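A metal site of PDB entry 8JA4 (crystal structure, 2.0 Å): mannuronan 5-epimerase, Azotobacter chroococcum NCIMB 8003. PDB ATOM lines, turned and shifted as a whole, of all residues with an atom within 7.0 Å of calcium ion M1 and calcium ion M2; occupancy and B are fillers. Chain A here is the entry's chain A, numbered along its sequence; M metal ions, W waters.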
ATOM      1  N   LEU A 321     -27.744 -23.548 -24.652  1.00  0.00           N
ATOM      2  CA  LEU A 321     -26.589 -23.238 -23.837  1.00  0.00           C
ATOM      3  C   LEU A 321     -26.109 -24.480 -23.115  1.00  0.00           C
ATOM      4  O   LEU A 321     -26.895 -25.411 -22.870  1.00  0.00           O
ATOM      5  CB  LEU A 321     -26.940 -22.221 -22.735  1.00  0.00           C
ATOM      6  CG  LEU A 321     -27.552 -20.917 -23.200  1.00  0.00           C
ATOM      7  CD1 LEU A 321     -28.315 -20.287 -22.052  1.00  0.00           C
ATOM      8  CD2 LEU A 321     -26.364 -20.029 -23.614  1.00  0.00           C
ATOM      9  N   ASN A 322     -24.909 -24.414 -22.542  1.00  0.00           N
ATOM     10  CA  ASN A 322     -24.400 -25.486 -21.646  1.00  0.00           C
ATOM     11  C   ASN A 322     -24.633 -26.862 -22.266  1.00  0.00           C
ATOM     12  O   ASN A 322     -25.296 -27.696 -21.638  1.00  0.00           O
ATOM     13  CB  ASN A 322     -24.983 -25.344 -20.245  1.00  0.00           C
ATOM     14  CG  ASN A 322     -24.765 -23.975 -19.625  1.00  0.00           C
ATOM     15  OD1 ASN A 322     -23.628 -23.540 -19.456  1.00  0.00           O
ATOM     16  ND2 ASN A 322     -25.845 -23.294 -19.276  1.00  0.00           N
ATOM     17  N   SER A 338     -23.916 -23.560 -30.080  1.00  0.00           N
ATOM     18  CA  SER A 338     -24.271 -23.195 -28.716  1.00  0.00           C
ATOM     19  C   SER A 338     -23.810 -21.755 -28.465  1.00  0.00           C
ATOM     20  O   SER A 338     -23.278 -21.060 -29.342  1.00  0.00           O
ATOM     21  CB  SER A 338     -23.666 -24.242 -27.764  1.00  0.00           C
ATOM     22  OG  SER A 338     -24.213 -24.036 -26.476  1.00  0.00           O
ATOM     23  N   SER A 339     -23.913 -21.280 -27.227  1.00  0.00           N
ATOM     24  CA  SER A 339     -23.757 -19.846 -26.922  1.00  0.00           C
ATOM     25  C   SER A 339     -22.941 -19.710 -25.636  1.00  0.00           C
ATOM     26  O   SER A 339     -22.094 -20.545 -25.330  1.00  0.00           O
ATOM     27  CB  SER A 339     -25.129 -19.165 -26.865  1.00  0.00           C
ATOM     28  OG  SER A 339     -24.979 -17.751 -26.910  1.00  0.00           O
ATOM     29  N   GLU A 340     -23.137 -18.564 -24.967  1.00  0.00           N
ATOM     30  CA  GLU A 340     -22.373 -18.222 -23.748  1.00  0.00           C
ATOM     31  C   GLU A 340     -22.117 -19.411 -22.743  1.00  0.00           C
ATOM     32  O   GLU A 340     -22.956 -20.304 -22.359  1.00  0.00           O
ATOM     33  CB  GLU A 340     -22.956 -17.016 -23.016  1.00  0.00           C
ATOM     34  CG  GLU A 340     -24.472 -16.974 -22.988  1.00  0.00           C
ATOM     35  CD  GLU A 340     -25.043 -15.971 -23.964  1.00  0.00           C
ATOM     36  OE1 GLU A 340     -25.965 -15.233 -23.571  1.00  0.00           O
ATOM     37  OE2 GLU A 340     -24.548 -15.914 -25.107  1.00  0.00           O
ATOM     38  N   GLY A 341     -20.885 -19.409 -22.249  1.00  0.00           N
ATOM     39  CA  GLY A 341     -20.520 -20.511 -21.386  1.00  0.00           C
ATOM     40  C   GLY A 341     -19.767 -21.586 -22.155  1.00  0.00           C
ATOM     41  O   GLY A 341     -19.618 -21.536 -23.372  1.00  0.00           O
ATOM     42  N   ARG A 342     -19.277 -22.569 -21.393  1.00  0.00           N
ATOM     43  CA  ARG A 342     -18.372 -23.601 -21.912  1.00  0.00           C
ATOM     44  C   ARG A 342     -19.189 -24.743 -22.504  1.00  0.00           C
ATOM     45  O   ARG A 342     -19.981 -25.363 -21.785  1.00  0.00           O
ATOM     46  CB  ARG A 342     -17.486 -24.104 -20.762  1.00  0.00           C
ATOM     47  CG  ARG A 342     -16.722 -25.389 -21.102  1.00  0.00           C
ATOM     48  CD  ARG A 342     -15.347 -25.359 -20.446  1.00  0.00           C
ATOM     49  NE  ARG A 342     -14.596 -26.579 -20.730  1.00  0.00           N
ATOM     50  CZ  ARG A 342     -13.905 -26.788 -21.855  1.00  0.00           C
ATOM     51  NH1 ARG A 342     -13.945 -25.906 -22.864  1.00  0.00           N
ATOM     52  NH2 ARG A 342     -13.155 -27.894 -21.967  1.00  0.00           N
ATOM     53  N   ASP A 343     -18.994 -25.029 -23.793  1.00  0.00           N
ATOM     54  CA  ASP A 343     -19.631 -26.156 -24.480  1.00  0.00           C
ATOM     55  C   ASP A 343     -18.603 -27.198 -24.892  1.00  0.00           C
ATOM     56  O   ASP A 343     -17.465 -26.870 -25.240  1.00  0.00           O
ATOM     57  CB  ASP A 343     -20.377 -25.634 -25.707  1.00  0.00           C
ATOM     58  CG  ASP A 343     -21.506 -24.676 -25.303  1.00  0.00           C
ATOM     59  OD1 ASP A 343     -22.628 -25.157 -24.985  1.00  0.00           O
ATOM     60  OD2 ASP A 343     -21.240 -23.447 -25.238  1.00  0.00           O
ATOM     61  N   LEU A 345     -18.371 -30.003 -27.697  1.00  0.00           N
ATOM     62  CA  LEU A 345     -19.147 -30.335 -28.900  1.00  0.00           C
ATOM     63  C   LEU A 345     -18.348 -31.285 -29.785  1.00  0.00           C
ATOM     64  O   LEU A 345     -17.361 -30.880 -30.419  1.00  0.00           O
ATOM     65  CB  LEU A 345     -19.537 -29.053 -29.649  1.00  0.00           C
ATOM     66  CG  LEU A 345     -20.351 -28.025 -28.841  1.00  0.00           C
ATOM     67  CD1 LEU A 345     -20.639 -26.739 -29.661  1.00  0.00           C
ATOM     68  CD2 LEU A 345     -21.667 -28.657 -28.402  1.00  0.00           C
ATOM     69  N   ASP A 355     -19.981 -24.756 -33.773  1.00  0.00           N
ATOM     70  CA  ASP A 355     -19.762 -23.383 -33.296  1.00  0.00           C
ATOM     71  C   ASP A 355     -20.196 -23.331 -31.834  1.00  0.00           C
ATOM     72  O   ASP A 355     -21.403 -23.293 -31.567  1.00  0.00           O
ATOM     73  CB  ASP A 355     -20.555 -22.363 -34.134  1.00  0.00           C
ATOM     74  CG  ASP A 355     -20.303 -20.895 -33.707  1.00  0.00           C
ATOM     75  OD1 ASP A 355     -19.703 -20.605 -32.617  1.00  0.00           O
ATOM     76  OD2 ASP A 355     -20.637 -19.998 -34.494  1.00  0.00           O
ATOM     77  N   GLY A 356     -19.238 -23.232 -30.902  1.00  0.00           N
ATOM     78  CA  GLY A 356     -19.585 -23.064 -29.482  1.00  0.00           C
ATOM     79  C   GLY A 356     -19.991 -21.662 -29.055  1.00  0.00           C
ATOM     80  O   GLY A 356     -20.329 -21.446 -27.864  1.00  0.00           O
ATOM     81  N   GLY A 357     -19.904 -20.678 -29.953  1.00  0.00           N
ATOM     82  CA  GLY A 357     -20.391 -19.350 -29.492  1.00  0.00           C
ATOM     83  C   GLY A 357     -19.497 -18.761 -28.408  1.00  0.00           C
ATOM     84  O   GLY A 357     -18.344 -19.155 -28.227  1.00  0.00           O
ATOM     85  N   ALA A 358     -20.030 -17.771 -27.675  1.00  0.00           N
ATOM     86  CA  ALA A 358     -19.251 -17.126 -26.611  1.00  0.00           C
ATOM     87  C   ALA A 358     -18.721 -18.141 -25.590  1.00  0.00           C
ATOM     88  O   ALA A 358     -19.217 -19.283 -25.496  1.00  0.00           O
ATOM     89  CB  ALA A 358     -20.121 -16.069 -25.917  1.00  0.00           C
ATOM     90  N   GLY A 359     -17.668 -17.760 -24.836  1.00  0.00           N
ATOM     91  CA  GLY A 359     -17.101 -18.636 -23.821  1.00  0.00           C
ATOM     92  C   GLY A 359     -16.144 -19.667 -24.400  1.00  0.00           C
ATOM     93  O   GLY A 359     -15.914 -19.748 -25.603  1.00  0.00           O
ATOM     94  N   ARG A 360     -15.593 -20.488 -23.504  1.00  0.00           N
ATOM     95  CA  ARG A 360     -14.463 -21.343 -23.852  1.00  0.00           C
ATOM     96  C   ARG A 360     -14.954 -22.746 -24.167  1.00  0.00           C
ATOM     97  O   ARG A 360     -15.327 -23.505 -23.261  1.00  0.00           O
ATOM     98  CB  ARG A 360     -13.414 -21.354 -22.737  1.00  0.00           C
ATOM     99  CG  ARG A 360     -12.171 -22.203 -23.120  1.00  0.00           C
ATOM    100  CD  ARG A 360     -11.146 -22.205 -21.973  1.00  0.00           C
ATOM    101  NE  ARG A 360     -11.523 -23.152 -20.928  1.00  0.00           N
ATOM    102  CZ  ARG A 360     -11.242 -24.462 -20.920  1.00  0.00           C
ATOM    103  NH1 ARG A 360     -10.588 -25.046 -21.924  1.00  0.00           N
ATOM    104  NH2 ARG A 360     -11.659 -25.203 -19.892  1.00  0.00           N
ATOM    105  N   ASP A 361     -14.900 -23.115 -25.433  1.00  0.00           N
ATOM    106  CA  ASP A 361     -15.440 -24.376 -25.920  1.00  0.00           C
ATOM    107  C   ASP A 361     -14.344 -25.327 -26.392  1.00  0.00           C
ATOM    108  O   ASP A 361     -13.275 -24.916 -26.850  1.00  0.00           O
ATOM    109  CB  ASP A 361     -16.359 -24.070 -27.090  1.00  0.00           C
ATOM    110  CG  ASP A 361     -17.290 -22.946 -26.776  1.00  0.00           C
ATOM    111  OD1 ASP A 361     -18.000 -23.093 -25.781  1.00  0.00           O
ATOM    112  OD2 ASP A 361     -17.320 -21.937 -27.511  1.00  0.00           O
ATOM    113  N   THR A 362     -14.653 -26.621 -26.337  1.00  0.00           N
ATOM    114  CA  THR A 362     -13.780 -27.668 -26.857  1.00  0.00           C
ATOM    115  C   THR A 362     -14.586 -28.390 -27.920  1.00  0.00           C
ATOM    116  O   THR A 362     -15.649 -28.941 -27.618  1.00  0.00           O
ATOM    117  CB  THR A 362     -13.352 -28.619 -25.739  1.00  0.00           C
ATOM    118  OG1 THR A 362     -12.660 -27.856 -24.734  1.00  0.00           O
ATOM    119  CG2 THR A 362     -12.416 -29.675 -26.271  1.00  0.00           C
ATOM    120  N   LEU A 363     -14.072 -28.381 -29.167  1.00  0.00           N
ATOM    121  CA  LEU A 363     -14.749 -28.868 -30.353  1.00  0.00           C
ATOM    122  C   LEU A 363     -13.936 -30.012 -30.965  1.00  0.00           C
ATOM    123  O   LEU A 363     -12.694 -29.992 -30.951  1.00  0.00           O
ATOM    124  CB  LEU A 363     -14.944 -27.751 -31.425  1.00  0.00           C
ATOM    125  CG  LEU A 363     -15.342 -26.390 -30.834  1.00  0.00           C
ATOM    126  CD1 LEU A 363     -15.134 -25.210 -31.796  1.00  0.00           C
ATOM    127  CD2 LEU A 363     -16.835 -26.458 -30.431  1.00  0.00           C
ATOM    128  N   PHE A 374     -16.302 -19.649 -36.271  1.00  0.00           N
ATOM    129  CA  PHE A 374     -16.080 -18.665 -35.218  1.00  0.00           C
ATOM    130  C   PHE A 374     -16.764 -17.396 -35.706  1.00  0.00           C
ATOM    131  O   PHE A 374     -16.301 -16.730 -36.642  1.00  0.00           O
ATOM    132  CB  PHE A 374     -14.581 -18.500 -34.940  1.00  0.00           C
ATOM    133  CG  PHE A 374     -13.969 -19.730 -34.368  1.00  0.00           C
ATOM    134  CD1 PHE A 374     -13.871 -19.890 -33.006  1.00  0.00           C
ATOM    135  CD2 PHE A 374     -13.583 -20.768 -35.202  1.00  0.00           C
ATOM    136  CE1 PHE A 374     -13.345 -21.083 -32.494  1.00  0.00           C
ATOM    137  CE2 PHE A 374     -13.088 -21.921 -34.716  1.00  0.00           C
ATOM    138  CZ  PHE A 374     -12.971 -22.095 -33.351  1.00  0.00           C
ATOM    139  N   GLN A 378     -15.008 -12.014 -30.273  1.00  0.00           N
ATOM    140  CA  GLN A 378     -15.072 -12.159 -28.826  1.00  0.00           C
ATOM    141  C   GLN A 378     -15.491 -13.578 -28.406  1.00  0.00           C
ATOM    142  O   GLN A 378     -15.670 -13.831 -27.232  1.00  0.00           O
ATOM    143  CB  GLN A 378     -16.010 -11.118 -28.203  1.00  0.00           C
ATOM    144  CG  GLN A 378     -15.499  -9.684 -28.266  1.00  0.00           C
ATOM    145  CD  GLN A 378     -14.228  -9.431 -27.419  1.00  0.00           C
ATOM    146  OE1 GLN A 378     -13.178  -8.937 -27.917  1.00  0.00           O
ATOM    147  NE2 GLN A 378     -14.336  -9.721 -26.104  1.00  0.00           N
ATOM    148  N   ASP A 379     -15.600 -14.512 -29.334  1.00  0.00           N
ATOM    149  CA  ASP A 379     -16.001 -15.869 -28.990  1.00  0.00           C
ATOM    150  C   ASP A 379     -14.842 -16.823 -28.681  1.00  0.00           C
ATOM    151  O   ASP A 379     -15.095 -17.971 -28.272  1.00  0.00           O
ATOM    152  CB  ASP A 379     -16.817 -16.472 -30.139  1.00  0.00           C
ATOM    153  CG  ASP A 379     -18.272 -15.904 -30.234  1.00  0.00           C
ATOM    154  OD1 ASP A 379     -18.738 -15.146 -29.303  1.00  0.00           O
ATOM    155  OD2 ASP A 379     -18.933 -16.259 -31.246  1.00  0.00           O
ATOM    156  N   SER A 380     -13.600 -16.397 -28.924  1.00  0.00           N
ATOM    157  CA  SER A 380     -12.425 -17.207 -28.626  1.00  0.00           C
ATOM    158  C   SER A 380     -11.311 -16.179 -28.519  1.00  0.00           C
ATOM    159  O   SER A 380     -10.945 -15.613 -29.554  1.00  0.00           O
ATOM    160  CB  SER A 380     -12.178 -18.235 -29.737  1.00  0.00           C
ATOM    161  OG  SER A 380     -11.121 -19.136 -29.383  1.00  0.00           O
ATOM    162  N   PHE A 381     -10.839 -15.905 -27.316  1.00  0.00           N
ATOM    163  CA  PHE A 381      -9.862 -14.807 -27.181  1.00  0.00           C
ATOM    164  C   PHE A 381      -8.993 -14.942 -25.934  1.00  0.00           C
ATOM    165  O   PHE A 381      -9.336 -15.698 -25.015  1.00  0.00           O
ATOM    166  CB  PHE A 381     -10.592 -13.470 -27.114  1.00  0.00           C
ATOM    167  CG  PHE A 381     -11.394 -13.263 -25.861  1.00  0.00           C
ATOM    168  CD1 PHE A 381     -12.688 -13.746 -25.770  1.00  0.00           C
ATOM    169  CD2 PHE A 381     -10.867 -12.587 -24.775  1.00  0.00           C
ATOM    170  CE1 PHE A 381     -13.436 -13.553 -24.616  1.00  0.00           C
ATOM    171  CE2 PHE A 381     -11.608 -12.394 -23.628  1.00  0.00           C
ATOM    172  CZ  PHE A 381     -12.889 -12.877 -23.552  1.00  0.00           C
ATOM    173  N   ARG A 390     -10.841 -18.521 -22.136  1.00  0.00           N
ATOM    174  CA  ARG A 390     -11.722 -17.954 -23.188  1.00  0.00           C
ATOM    175  C   ARG A 390     -11.142 -18.307 -24.556  1.00  0.00           C
ATOM    176  O   ARG A 390     -11.733 -17.892 -25.560  1.00  0.00           O
ATOM    177  CB  ARG A 390     -11.915 -16.451 -22.972  1.00  0.00           C
ATOM    178  CG  ARG A 390     -12.434 -16.093 -21.578  1.00  0.00           C
ATOM    179  CD  ARG A 390     -13.473 -17.082 -21.092  1.00  0.00           C
ATOM    180  NE  ARG A 390     -13.388 -17.275 -19.649  1.00  0.00           N
ATOM    181  CZ  ARG A 390     -13.557 -16.307 -18.748  1.00  0.00           C
ATOM    182  NH1 ARG A 390     -13.815 -15.078 -19.147  1.00  0.00           N
ATOM    183  NH2 ARG A 390     -13.469 -16.576 -17.463  1.00  0.00           N
ATOM    184  N   VAL A 391     -10.056 -19.073 -24.597  1.00  0.00           N
ATOM    185  CA  VAL A 391      -9.511 -19.543 -25.905  1.00  0.00           C
ATOM    186  C   VAL A 391     -10.071 -20.935 -26.213  1.00  0.00           C
ATOM    187  O   VAL A 391      -9.742 -21.873 -25.483  1.00  0.00           O
ATOM    188  CB  VAL A 391      -7.968 -19.534 -25.961  1.00  0.00           C
ATOM    189  CG1 VAL A 391      -7.468 -20.155 -27.244  1.00  0.00           C
ATOM    190  CG2 VAL A 391      -7.412 -18.126 -25.801  1.00  0.00           C
ATOM    191  N   ASP A 392     -10.880 -21.032 -27.254  1.00  0.00           N
ATOM    192  CA  ASP A 392     -11.406 -22.310 -27.717  1.00  0.00           C
ATOM    193  C   ASP A 392     -10.280 -23.259 -28.175  1.00  0.00           C
ATOM    194  O   ASP A 392      -9.269 -22.825 -28.762  1.00  0.00           O
ATOM    195  CB  ASP A 392     -12.347 -22.120 -28.906  1.00  0.00           C
ATOM    196  CG  ASP A 392     -13.704 -21.529 -28.521  1.00  0.00           C
ATOM    197  OD1 ASP A 392     -13.923 -21.035 -27.394  1.00  0.00           O
ATOM    198  OD2 ASP A 392     -14.604 -21.619 -29.390  1.00  0.00           O
HETATM  199 CA    CA M   1     -16.095 -20.015 -28.047  1.00  0.00          CA
HETATM  200 CA    CA M   2     -19.918 -21.547 -25.625  1.00  0.00          CA
HETATM  201  O   HOH W   1     -16.490 -19.928 -30.405  1.00  0.00           O
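OD1 of Asp 379 sits at hydrogen-bond distance from N of Ala 358, at 3.3 Å.
OG of Ser 338 lies within hydrogen-bond range of OD1 of Asp 343, 2.4 Å away.
The side-chain carboxylate of Asp 343 sits at hydrogen-bond distance from the backbone NH of Asn 322 (3.4 Å).
The backbone carbonyl oxygen of Asp 343 is in hydrogen-bond range of the backbone NH of Thr 362, 3.0 Å away.
OE2 of Glu 340 is in hydrogen-bond range of OG of Ser 339, 2.6 Å away.
The backbone NH of Gly 357 sits close to the backbone carbonyl oxygen of Ser 338.
The side-chain carboxylate (OD1) of Asp 355 sits at hydrogen-bond distance from the backbone NH (N) of Gly 357, at 2.7 Å.
N of Asp 392 lies within hydrogen-bond range of OG of Ser 380, at 2.9 Å.
Calcium ion M2 is bound by the backbone carbonyl oxygen (O) of Gly 341 (2.3 Å), the backbone carbonyl oxygen (O) of Gly 356 (2.3 Å), the side-chain carboxylate (OD2) of Asp 343 (2.3 Å), the backbone carbonyl oxygen (O) of Ala 358 (2.4 Å), the backbone carbonyl oxygen (O) of Ser 339 (2.4 Å) and the side-chain carboxylate (OD1) of Asp 361 (2.5 Å).
Calcium ion M2 has six donor atoms within binding distance.
Within 4 Å of calcium ion M1: Gly 357, Gly 359, Asp 361, Asp 379 and Asp 392.
The nearest printed residue that does not touch calcium ion M1 is Ala 358 (4.1 Å).
The nearest printed residue that does not touch calcium ion M2 is Glu 340 (4.2 Å).
Calcium ion M1 is bound by the backbone carbonyl oxygen (O) of Asp 379 (2.3 Å).
OD2 of Asp 361 binds calcium ion M1.
Water W1 is bound to calcium ion M1 (2.4 Å).
The backbone carbonyl oxygen (O) of Gly 357 is bound to calcium ion M1, at 2.4 Å.
The backbone carbonyl oxygen (O) of Gly 359 is bound to calcium ion M1.
OD1 of Asp 392 is bound to calcium ion M1.
OD2 of Asp 392 is bound to calcium ion M1 (2.6 Å).
Calcium ion M1 has seven donor atoms within binding distance.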
